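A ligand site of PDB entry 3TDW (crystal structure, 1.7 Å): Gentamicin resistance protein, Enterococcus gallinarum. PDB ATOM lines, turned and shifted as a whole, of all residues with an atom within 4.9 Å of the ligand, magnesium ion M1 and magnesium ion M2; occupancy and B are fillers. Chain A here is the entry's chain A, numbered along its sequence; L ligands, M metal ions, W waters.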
ATOM      1  N   LEU A  27      21.760  19.518 -11.533  1.00  0.00           N
ATOM      2  CA  LEU A  27      20.470  19.854 -12.128  1.00  0.00           C
ATOM      3  C   LEU A  27      19.533  18.653 -12.059  1.00  0.00           C
ATOM      4  O   LEU A  27      18.358  18.798 -11.739  1.00  0.00           O
ATOM      5  CB  LEU A  27      20.647  20.316 -13.574  1.00  0.00           C
ATOM      6  CG  LEU A  27      19.345  20.563 -14.309  1.00  0.00           C
ATOM      7  CD1 LEU A  27      18.575  21.705 -13.633  1.00  0.00           C
ATOM      8  CD2 LEU A  27      19.594  20.886 -15.785  1.00  0.00           C
ATOM      9  N   GLY A  28      20.062  17.477 -12.357  1.00  0.00           N
ATOM     10  CA  GLY A  28      19.257  16.265 -12.383  1.00  0.00           C
ATOM     11  C   GLY A  28      20.066  15.071 -12.844  1.00  0.00           C
ATOM     12  O   GLY A  28      21.213  15.190 -13.299  1.00  0.00           O
ATOM     13  N   GLU A  29      19.479  13.888 -12.700  1.00  0.00           N
ATOM     14  CA  GLU A  29      20.177  12.676 -12.994  1.00  0.00           C
ATOM     15  C   GLU A  29      19.145  11.628 -13.340  1.00  0.00           C
ATOM     16  O   GLU A  29      18.073  11.594 -12.739  1.00  0.00           O
ATOM     17  CB  GLU A  29      20.960  12.248 -11.746  1.00  0.00           C
ATOM     18  CG  GLU A  29      21.933  11.113 -11.923  1.00  0.00           C
ATOM     19  CD  GLU A  29      22.594  10.722 -10.618  1.00  0.00           C
ATOM     20  OE1 GLU A  29      22.304  11.372  -9.586  1.00  0.00           O
ATOM     21  OE2 GLU A  29      23.399   9.768 -10.612  1.00  0.00           O
ATOM     22  N   GLY A  30      19.462  10.776 -14.308  1.00  0.00           N
ATOM     23  CA  GLY A  30      18.667   9.602 -14.603  1.00  0.00           C
ATOM     24  C   GLY A  30      19.529   8.366 -14.550  1.00  0.00           C
ATOM     25  O   GLY A  30      20.624   8.367 -13.964  1.00  0.00           O
ATOM     26  N   PHE A  31      19.051   7.291 -15.158  1.00  0.00           N
ATOM     27  CA  PHE A  31      19.843   6.065 -15.214  1.00  0.00           C
ATOM     28  C   PHE A  31      21.025   6.155 -16.174  1.00  0.00           C
ATOM     29  O   PHE A  31      21.964   5.367 -16.059  1.00  0.00           O
ATOM     30  CB  PHE A  31      18.967   4.881 -15.622  1.00  0.00           C
ATOM     31  CG  PHE A  31      18.055   4.384 -14.536  1.00  0.00           C
ATOM     32  CD1 PHE A  31      16.843   5.000 -14.306  1.00  0.00           C
ATOM     33  CD2 PHE A  31      18.381   3.271 -13.780  1.00  0.00           C
ATOM     34  CE1 PHE A  31      15.989   4.548 -13.304  1.00  0.00           C
ATOM     35  CE2 PHE A  31      17.536   2.808 -12.789  1.00  0.00           C
ATOM     36  CZ  PHE A  31      16.346   3.448 -12.548  1.00  0.00           C
ATOM     37  N   ARG A  32      20.977   7.084 -17.130  1.00  0.00           N
ATOM     38  CA  ARG A  32      21.976   7.103 -18.210  1.00  0.00           C
ATOM     39  C   ARG A  32      22.905   8.299 -18.151  1.00  0.00           C
ATOM     40  O   ARG A  32      24.030   8.208 -18.654  1.00  0.00           O
ATOM     41  CB  ARG A  32      21.273   7.118 -19.586  1.00  0.00           C
ATOM     42  CG  ARG A  32      20.396   5.890 -19.852  1.00  0.00           C
ATOM     43  CD  ARG A  32      21.198   4.621 -20.269  1.00  0.00           C
ATOM     44  NE  ARG A  32      20.224   3.586 -20.631  1.00  0.00           N
ATOM     45  CZ  ARG A  32      19.756   2.671 -19.786  1.00  0.00           C
ATOM     46  NH1 ARG A  32      20.221   2.601 -18.539  1.00  0.00           N
ATOM     47  NH2 ARG A  32      18.823   1.806 -20.194  1.00  0.00           N
ATOM     48  N   ASN A  33      22.437   9.396 -17.555  1.00  0.00           N
ATOM     49  CA  ASN A  33      23.158  10.678 -17.560  1.00  0.00           C
ATOM     50  C   ASN A  33      23.099  11.441 -16.259  1.00  0.00           C
ATOM     51  O   ASN A  33      22.094  11.425 -15.552  1.00  0.00           O
ATOM     52  CB  ASN A  33      22.588  11.598 -18.652  1.00  0.00           C
ATOM     53  CG  ASN A  33      22.823  11.052 -20.030  1.00  0.00           C
ATOM     54  OD1 ASN A  33      23.911  11.157 -20.561  1.00  0.00           O
ATOM     55  ND2 ASN A  33      21.783  10.488 -20.631  1.00  0.00           N
ATOM     56  N   ALA A  35      23.368  15.428 -15.102  1.00  0.00           N
ATOM     57  CA  ALA A  35      23.294  16.765 -15.683  1.00  0.00           C
ATOM     58  C   ALA A  35      23.617  17.867 -14.674  1.00  0.00           C
ATOM     59  O   ALA A  35      23.101  17.871 -13.564  1.00  0.00           O
ATOM     60  CB  ALA A  35      21.916  17.008 -16.315  1.00  0.00           C
ATOM     61  N   VAL A  43      23.120  23.546 -19.757  1.00  0.00           N
ATOM     62  CA  VAL A  43      23.103  22.181 -19.252  1.00  0.00           C
ATOM     63  C   VAL A  43      24.248  21.403 -19.848  1.00  0.00           C
ATOM     64  O   VAL A  43      24.386  21.334 -21.072  1.00  0.00           O
ATOM     65  CB  VAL A  43      21.800  21.441 -19.626  1.00  0.00           C
ATOM     66  CG1 VAL A  43      21.830  20.006 -19.072  1.00  0.00           C
ATOM     67  CG2 VAL A  43      20.585  22.221 -19.138  1.00  0.00           C
ATOM     68  N   ARG A  45      25.727  17.548 -19.876  1.00  0.00           N
ATOM     69  CA  ARG A  45      25.119  16.269 -19.598  1.00  0.00           C
ATOM     70  C   ARG A  45      26.131  15.163 -19.894  1.00  0.00           C
ATOM     71  O   ARG A  45      26.618  15.044 -21.022  1.00  0.00           O
ATOM     72  CB  ARG A  45      23.865  16.140 -20.458  1.00  0.00           C
ATOM     73  CG  ARG A  45      23.046  14.878 -20.307  1.00  0.00           C
ATOM     74  CD  ARG A  45      21.847  15.061 -21.216  1.00  0.00           C
ATOM     75  NE  ARG A  45      20.901  13.949 -21.324  1.00  0.00           N
ATOM     76  CZ  ARG A  45      20.805  13.161 -22.394  1.00  0.00           C
ATOM     77  NH1 ARG A  45      21.650  13.318 -23.404  1.00  0.00           N
ATOM     78  NH2 ARG A  45      19.853  12.226 -22.454  1.00  0.00           N
ATOM     79  N   GLU A  55      23.494   5.830 -26.405  1.00  0.00           N
ATOM     80  CA  GLU A  55      22.251   6.585 -26.583  1.00  0.00           C
ATOM     81  C   GLU A  55      22.558   8.051 -26.947  1.00  0.00           C
ATOM     82  O   GLU A  55      21.931   8.631 -27.809  1.00  0.00           O
ATOM     83  CB  GLU A  55      21.348   6.481 -25.348  1.00  0.00           C
ATOM     84  CG  GLU A  55      20.888   5.040 -25.085  1.00  0.00           C
ATOM     85  CD  GLU A  55      20.014   4.860 -23.836  1.00  0.00           C
ATOM     86  OE1 GLU A  55      19.554   5.858 -23.228  1.00  0.00           O
ATOM     87  OE2 GLU A  55      19.766   3.704 -23.460  1.00  0.00           O
ATOM     88  N   TYR A  92      24.086  22.061 -23.737  1.00  0.00           N
ATOM     89  CA  TYR A  92      23.014  22.753 -24.460  1.00  0.00           C
ATOM     90  C   TYR A  92      22.357  23.842 -23.638  1.00  0.00           C
ATOM     91  O   TYR A  92      22.402  23.785 -22.411  1.00  0.00           O
ATOM     92  CB  TYR A  92      21.957  21.774 -24.966  1.00  0.00           C
ATOM     93  CG  TYR A  92      21.330  20.807 -23.948  1.00  0.00           C
ATOM     94  CD1 TYR A  92      21.898  19.568 -23.715  1.00  0.00           C
ATOM     95  CD2 TYR A  92      20.129  21.112 -23.300  1.00  0.00           C
ATOM     96  CE1 TYR A  92      21.309  18.660 -22.819  1.00  0.00           C
ATOM     97  CE2 TYR A  92      19.551  20.215 -22.398  1.00  0.00           C
ATOM     98  CZ  TYR A  92      20.137  18.988 -22.172  1.00  0.00           C
ATOM     99  OH  TYR A  92      19.554  18.067 -21.296  1.00  0.00           O
ATOM    100  N   LYS A  94      19.717  25.454 -21.594  1.00  0.00           N
ATOM    101  CA  LYS A  94      18.631  24.867 -20.795  1.00  0.00           C
ATOM    102  C   LYS A  94      17.291  25.024 -21.497  1.00  0.00           C
ATOM    103  O   LYS A  94      16.944  26.108 -21.982  1.00  0.00           O
ATOM    104  CB  LYS A  94      18.567  25.575 -19.443  1.00  0.00           C
ATOM    105  CG  LYS A  94      17.793  24.858 -18.350  1.00  0.00           C
ATOM    106  CD  LYS A  94      17.641  25.785 -17.132  1.00  0.00           C
ATOM    107  CE  LYS A  94      17.139  25.025 -15.915  1.00  0.00           C
ATOM    108  NZ  LYS A  94      16.501  25.917 -14.902  1.00  0.00           N
ATOM    109  N   VAL A  95      16.531  23.932 -21.562  1.00  0.00           N
ATOM    110  CA  VAL A  95      15.148  23.995 -22.011  1.00  0.00           C
ATOM    111  C   VAL A  95      14.369  24.602 -20.837  1.00  0.00           C
ATOM    112  O   VAL A  95      14.325  24.037 -19.734  1.00  0.00           O
ATOM    113  CB  VAL A  95      14.604  22.601 -22.379  1.00  0.00           C
ATOM    114  CG1 VAL A  95      13.114  22.689 -22.794  1.00  0.00           C
ATOM    115  CG2 VAL A  95      15.455  21.948 -23.481  1.00  0.00           C
ATOM    116  N   GLY A  97      11.518  26.244 -18.254  1.00  0.00           N
ATOM    117  CA  GLY A  97      10.263  25.818 -17.675  1.00  0.00           C
ATOM    118  C   GLY A  97      10.508  25.002 -16.421  1.00  0.00           C
ATOM    119  O   GLY A  97      11.665  24.771 -16.036  1.00  0.00           O
ATOM    120  N   ILE A  99       9.943  21.286 -14.624  1.00  0.00           N
ATOM    121  CA  ILE A  99       9.646  19.881 -14.918  1.00  0.00           C
ATOM    122  C   ILE A  99       8.320  19.496 -14.285  1.00  0.00           C
ATOM    123  O   ILE A  99       8.157  19.602 -13.071  1.00  0.00           O
ATOM    124  CB  ILE A  99      10.716  18.960 -14.328  1.00  0.00           C
ATOM    125  CG1 ILE A  99      12.092  19.270 -14.942  1.00  0.00           C
ATOM    126  CG2 ILE A  99      10.334  17.488 -14.528  1.00  0.00           C
ATOM    127  CD1 ILE A  99      12.503  18.318 -16.045  1.00  0.00           C
ATOM    128  N   ASP A 196      10.741   7.722 -24.274  1.00  0.00           N
ATOM    129  CA  ASP A 196      10.781   8.003 -22.845  1.00  0.00           C
ATOM    130  C   ASP A 196       9.869   9.189 -22.545  1.00  0.00           C
ATOM    131  O   ASP A 196      10.231  10.128 -21.814  1.00  0.00           O
ATOM    132  CB  ASP A 196      12.229   8.289 -22.401  1.00  0.00           C
ATOM    133  CG  ASP A 196      12.527   7.768 -21.005  1.00  0.00           C
ATOM    134  OD1 ASP A 196      11.580   7.341 -20.317  1.00  0.00           O
ATOM    135  OD2 ASP A 196      13.709   7.784 -20.600  1.00  0.00           O
ATOM    136  N   ASP A 200       8.368  13.564 -16.418  1.00  0.00           N
ATOM    137  CA  ASP A 200       9.676  14.000 -15.887  1.00  0.00           C
ATOM    138  C   ASP A 200      10.534  14.621 -16.998  1.00  0.00           C
ATOM    139  O   ASP A 200      11.629  15.137 -16.748  1.00  0.00           O
ATOM    140  CB  ASP A 200      10.428  12.878 -15.166  1.00  0.00           C
ATOM    141  CG  ASP A 200       9.698  12.383 -13.939  1.00  0.00           C
ATOM    142  OD1 ASP A 200       9.693  11.156 -13.719  1.00  0.00           O
ATOM    143  OD2 ASP A 200       9.124  13.215 -13.205  1.00  0.00           O
ATOM    144  N   HIS A 201      10.038  14.569 -18.229  1.00  0.00           N
ATOM    145  CA  HIS A 201      10.724  15.172 -19.367  1.00  0.00           C
ATOM    146  C   HIS A 201       9.919  16.290 -20.011  1.00  0.00           C
ATOM    147  O   HIS A 201      10.263  16.740 -21.102  1.00  0.00           O
ATOM    148  CB  HIS A 201      11.032  14.135 -20.441  1.00  0.00           C
ATOM    149  CG  HIS A 201      11.997  13.076 -20.003  1.00  0.00           C
ATOM    150  ND1 HIS A 201      11.930  11.779 -20.465  1.00  0.00           N
ATOM    151  CD2 HIS A 201      13.039  13.117 -19.138  1.00  0.00           C
ATOM    152  CE1 HIS A 201      12.898  11.068 -19.910  1.00  0.00           C
ATOM    153  NE2 HIS A 201      13.577  11.851 -19.103  1.00  0.00           N
ATOM    154  N   LEU A 203       8.698  20.057 -19.964  1.00  0.00           N
ATOM    155  CA  LEU A 203       9.080  21.351 -19.405  1.00  0.00           C
ATOM    156  C   LEU A 203       7.912  22.290 -19.618  1.00  0.00           C
ATOM    157  O   LEU A 203       7.461  22.477 -20.750  1.00  0.00           O
ATOM    158  CB  LEU A 203      10.317  21.891 -20.111  1.00  0.00           C
ATOM    159  CG  LEU A 203      11.646  21.417 -19.516  1.00  0.00           C
ATOM    160  CD1 LEU A 203      11.771  21.868 -18.081  1.00  0.00           C
ATOM    161  CD2 LEU A 203      11.811  19.903 -19.609  1.00  0.00           C
ATOM    162  N   ILE A 217      12.620  16.941 -23.169  1.00  0.00           N
ATOM    163  CA  ILE A 217      14.027  16.577 -23.121  1.00  0.00           C
ATOM    164  C   ILE A 217      14.239  15.054 -23.236  1.00  0.00           C
ATOM    165  O   ILE A 217      13.285  14.295 -23.425  1.00  0.00           O
ATOM    166  CB  ILE A 217      14.682  17.084 -21.830  1.00  0.00           C
ATOM    167  CG1 ILE A 217      13.944  16.528 -20.602  1.00  0.00           C
ATOM    168  CG2 ILE A 217      14.684  18.624 -21.803  1.00  0.00           C
ATOM    169  CD1 ILE A 217      14.732  16.683 -19.304  1.00  0.00           C
ATOM    170  N   ASP A 218      15.510  14.637 -23.124  1.00  0.00           N
ATOM    171  CA  ASP A 218      15.926  13.232 -23.069  1.00  0.00           C
ATOM    172  C   ASP A 218      15.430  12.325 -24.186  1.00  0.00           C
ATOM    173  O   ASP A 218      14.493  11.543 -24.001  1.00  0.00           O
ATOM    174  CB  ASP A 218      15.565  12.580 -21.726  1.00  0.00           C
ATOM    175  CG  ASP A 218      16.310  11.284 -21.499  1.00  0.00           C
ATOM    176  OD1 ASP A 218      17.211  10.944 -22.314  1.00  0.00           O
ATOM    177  OD2 ASP A 218      16.038  10.597 -20.496  1.00  0.00           O
ATOM    178  N   GLY A 220      17.138   9.859 -25.484  1.00  0.00           N
ATOM    179  CA  GLY A 220      18.062   8.715 -25.533  1.00  0.00           C
ATOM    180  C   GLY A 220      17.415   7.390 -25.926  1.00  0.00           C
ATOM    181  O   GLY A 220      18.095   6.458 -26.392  1.00  0.00           O
ATOM    182  N   ASP A 221      16.106   7.266 -25.731  1.00  0.00           N
ATOM    183  CA  ASP A 221      15.417   6.030 -26.106  1.00  0.00           C
ATOM    184  C   ASP A 221      14.698   6.098 -27.454  1.00  0.00           C
ATOM    185  O   ASP A 221      13.891   5.223 -27.779  1.00  0.00           O
ATOM    186  CB  ASP A 221      14.455   5.582 -25.004  1.00  0.00           C
ATOM    187  CG  ASP A 221      15.184   4.915 -23.853  1.00  0.00           C
ATOM    188  OD1 ASP A 221      15.818   3.857 -24.081  1.00  0.00           O
ATOM    189  OD2 ASP A 221      15.152   5.456 -22.725  1.00  0.00           O
HETATM  190  P1  LIG L   1      18.734  10.316 -18.360  1.00  0.00           P
HETATM  191  O1  LIG L   1      19.711   9.630 -17.447  1.00  0.00           O
HETATM  192  O2  LIG L   1      17.358  10.011 -17.861  1.00  0.00           O
HETATM  193  O3  LIG L   1      18.942   9.915 -19.772  1.00  0.00           O
HETATM  194  O4  LIG L   1      19.039  11.914 -18.231  1.00  0.00           O
HETATM  195  P2  LIG L   1      18.150  13.136 -18.786  1.00  0.00           P
HETATM  196  O5  LIG L   1      18.445  13.564 -20.184  1.00  0.00           O
HETATM  197  O6  LIG L   1      16.679  12.850 -18.568  1.00  0.00           O
HETATM  198  O7  LIG L   1      18.584  14.308 -17.774  1.00  0.00           O
HETATM  199  C1  LIG L   1      18.571  14.036 -16.377  1.00  0.00           C
HETATM  200  C2  LIG L   1      17.745  15.098 -15.653  1.00  0.00           C
HETATM  201  O8  LIG L   1      18.368  16.370 -15.757  1.00  0.00           O
HETATM  202  C3  LIG L   1      16.358  15.295 -16.246  1.00  0.00           C
HETATM  203  O9  LIG L   1      15.460  14.291 -15.757  1.00  0.00           O
HETATM  204  C4  LIG L   1      16.020  16.675 -15.734  1.00  0.00           C
HETATM  205  O10 LIG L   1      15.607  16.547 -14.370  1.00  0.00           O
HETATM  206  C5  LIG L   1      17.359  17.386 -15.782  1.00  0.00           C
HETATM  207  N1  LIG L   1      17.465  18.127 -17.052  1.00  0.00           N
HETATM  208  C6  LIG L   1      18.133  17.751 -18.168  1.00  0.00           C
HETATM  209  N2  LIG L   1      18.006  18.681 -19.146  1.00  0.00           N
HETATM  210  C7  LIG L   1      17.230  19.670 -18.643  1.00  0.00           C
HETATM  211  C8  LIG L   1      16.736  20.974 -19.133  1.00  0.00           C
HETATM  212  O11 LIG L   1      16.985  21.358 -20.284  1.00  0.00           O
HETATM  213  N3  LIG L   1      15.977  21.703 -18.295  1.00  0.00           N
HETATM  214  C9  LIG L   1      15.706  21.290 -17.041  1.00  0.00           C
HETATM  215  N4  LIG L   1      14.944  22.084 -16.243  1.00  0.00           N
HETATM  216  N5  LIG L   1      16.147  20.126 -16.526  1.00  0.00           N
HETATM  217  C10 LIG L   1      16.903  19.297 -17.276  1.00  0.00           C
HETATM  218 MG    MG M   1      15.591  11.073 -18.398  1.00  0.00          MG
HETATM  219 MG    MG M   2      17.632   9.087 -21.100  1.00  0.00          MG
HETATM  220  O   HOH W   1      15.995   8.129 -22.275  1.00  0.00           O
HETATM  221  O   HOH W   2      15.830  18.846 -12.686  1.00  0.00           O
HETATM  222  O   HOH W   3      19.188   8.262 -22.430  1.00  0.00           O
HETATM  223  O   HOH W   4      14.589   9.056 -18.184  1.00  0.00           O
HETATM  224  O   HOH W   5      18.177  15.653 -22.075  1.00  0.00           O
HETATM  225  O   HOH W   6      15.002  11.616 -16.316  1.00  0.00           O
HETATM  226  O   HOH W   7      14.639  21.323 -13.283  1.00  0.00           O
HETATM  227  O   HOH W   8      16.881   7.630 -16.936  1.00  0.00           O
HETATM  228  O   HOH W   9      17.397   7.487 -19.736  1.00  0.00           O
HETATM  229  O   HOH W  10      13.114  15.114 -14.403  1.00  0.00           O
HETATM  230  O   HOH W  11      16.490  14.411 -11.962  1.00  0.00           O
HETATM  231  O   HOH W  12      14.255  24.700 -17.029  1.00  0.00           O
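N of Phe 31 lies within hydrogen-bond range of O1 of the ligand (3.3 Å).
A nitrogen (N2) of the ligand is in hydrogen-bond range of the side-chain hydroxyl of Tyr 92 (2.7 Å).
The backbone NH (N) of Gly 30 lies close to an oxygen (O1) of the ligand (3.4 Å).
An oxygen (O1) of the ligand is in hydrogen-bond range of the backbone NH of Asn 33.
The backbone carbonyl oxygen of Val 95 lies within hydrogen-bond range of a nitrogen (N3) of the ligand (3.2 Å).
ND2 of Asn 33 sits close to O3 of the ligand (3.0 Å).
O11 of the ligand sits at hydrogen-bond distance from N of Val 95.
The backbone NH (N) of Arg 32 lies within hydrogen-bond range of an oxygen (O1) of the ligand (2.9 Å).
The guanidinium group of Arg 45 is in salt-bridge range of an oxygen (O5) of the ligand, 2.7 Å away.
A ring nitrogen (ND1) of His 201 sits at hydrogen-bond distance from the backbone carbonyl oxygen of Asp 196 (2.7 Å).
The guanidinium group of Arg 32 is in salt-bridge range of the side-chain carboxylate of Glu 55, 3.5 Å away.
O of His 201 sits at hydrogen-bond distance from N of Ile 217 (3.1 Å).
The side-chain carboxylate of Asp 218 sits close to the backbone NH of Gly 220, 3.4 Å away.
O of Ala 35 is in hydrogen-bond range of N of Leu 27, at 2.9 Å.
NH2 of Arg 45 lies close to ND2 of Asn 33, at 3.2 Å.
NH2 of Arg 45 lies close to OD1 of Asp 218 (2.9 Å).
The backbone carbonyl oxygen (O) of Gly 28 lies within hydrogen-bond range of the backbone NH (N) of Ala 35 (2.8 Å).
Merely in contact with the ligand: Leu 27, Gly 28, Glu 29, Ala 35, Val 43, Lys 94, Ile 99, Leu 203 and Ile 217.
Hydrophobic or aromatic side chains that line the ligand: Leu 27, Ala 35, Val 43, Tyr 92, Val 95, Ile 99, His 201, Leu 203 and Ile 217.
Within 4 Å of the ligand: Leu 27, Gly 28, Glu 29, Gly 30, Phe 31, Arg 32, Asn 33, Ala 35, Val 43, Arg 45, Tyr 92, Lys 94, Val 95, Ile 99, His 201, Leu 203, Ile 217 and Asp 218.
Within 4 Å of magnesium ion M1: His 201 and Asp 218.
The nearest printed residue that does not touch magnesium ion M1 is Asp 196 (4.4 Å).
One residue has an atom within 4 Å of magnesium ion M2: Asp 218.
Magnesium ion M1 is bound by O6 of the ligand, at 2.1 Å.
Magnesium ion M1 is bound by O2 of the ligand (2.1 Å).
The side-chain carboxylate (OD2) of Asp 218 binds magnesium ion M1, at 2.2 Å.
Water W6 binds magnesium ion M1, at 2.2 Å.
Water W4 is bound to magnesium ion M1.
Magnesium ion M1 is bound by NE2 of His 201, at 2.3 Å.
Magnesium ion M2 is bound by O3 of the ligand (2.0 Å), water W9 (2.1 Å), water W3 (2.2 Å), water W1 (2.2 Å), OD1 of Asp 218 (2.3 Å) and OD2 of Asp 218 (2.3 Å).
Magnesium ion M2 has six donor atoms within binding distance.
Water W1 lies within hydrogen-bond range of OD2 of Asp 221 (2.8 Å) and OD2 of Asp 196 (2.9 Å).
Water W12 lies within hydrogen-bond range of the backbone carbonyl oxygen of Gly 97 (2.8 Å), the backbone carbonyl oxygen of Val 95 (2.8 Å), a nitrogen (N4) of the ligand (2.8 Å) and the side-chain amino group of Lys 94 (3.3 Å).
Water W5 lies within hydrogen-bond range of O5 of the ligand (2.8 Å), OH of Tyr 92 (2.9 Å), N of Asp 218 (3.0 Å) and NE of Arg 45 (3.3 Å).
Water W10 bridges O of Asp 200 and O9 of the ligand.
Water W2 bridges the backbone carbonyl oxygen (O) of Leu 27 (2.7 Å) and an oxygen (O10) of the ligand (2.9 Å).
Water W11 lies within hydrogen-bond range of N of Glu 29 (3.1 Å) and O10 of the ligand (3.3 Å).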
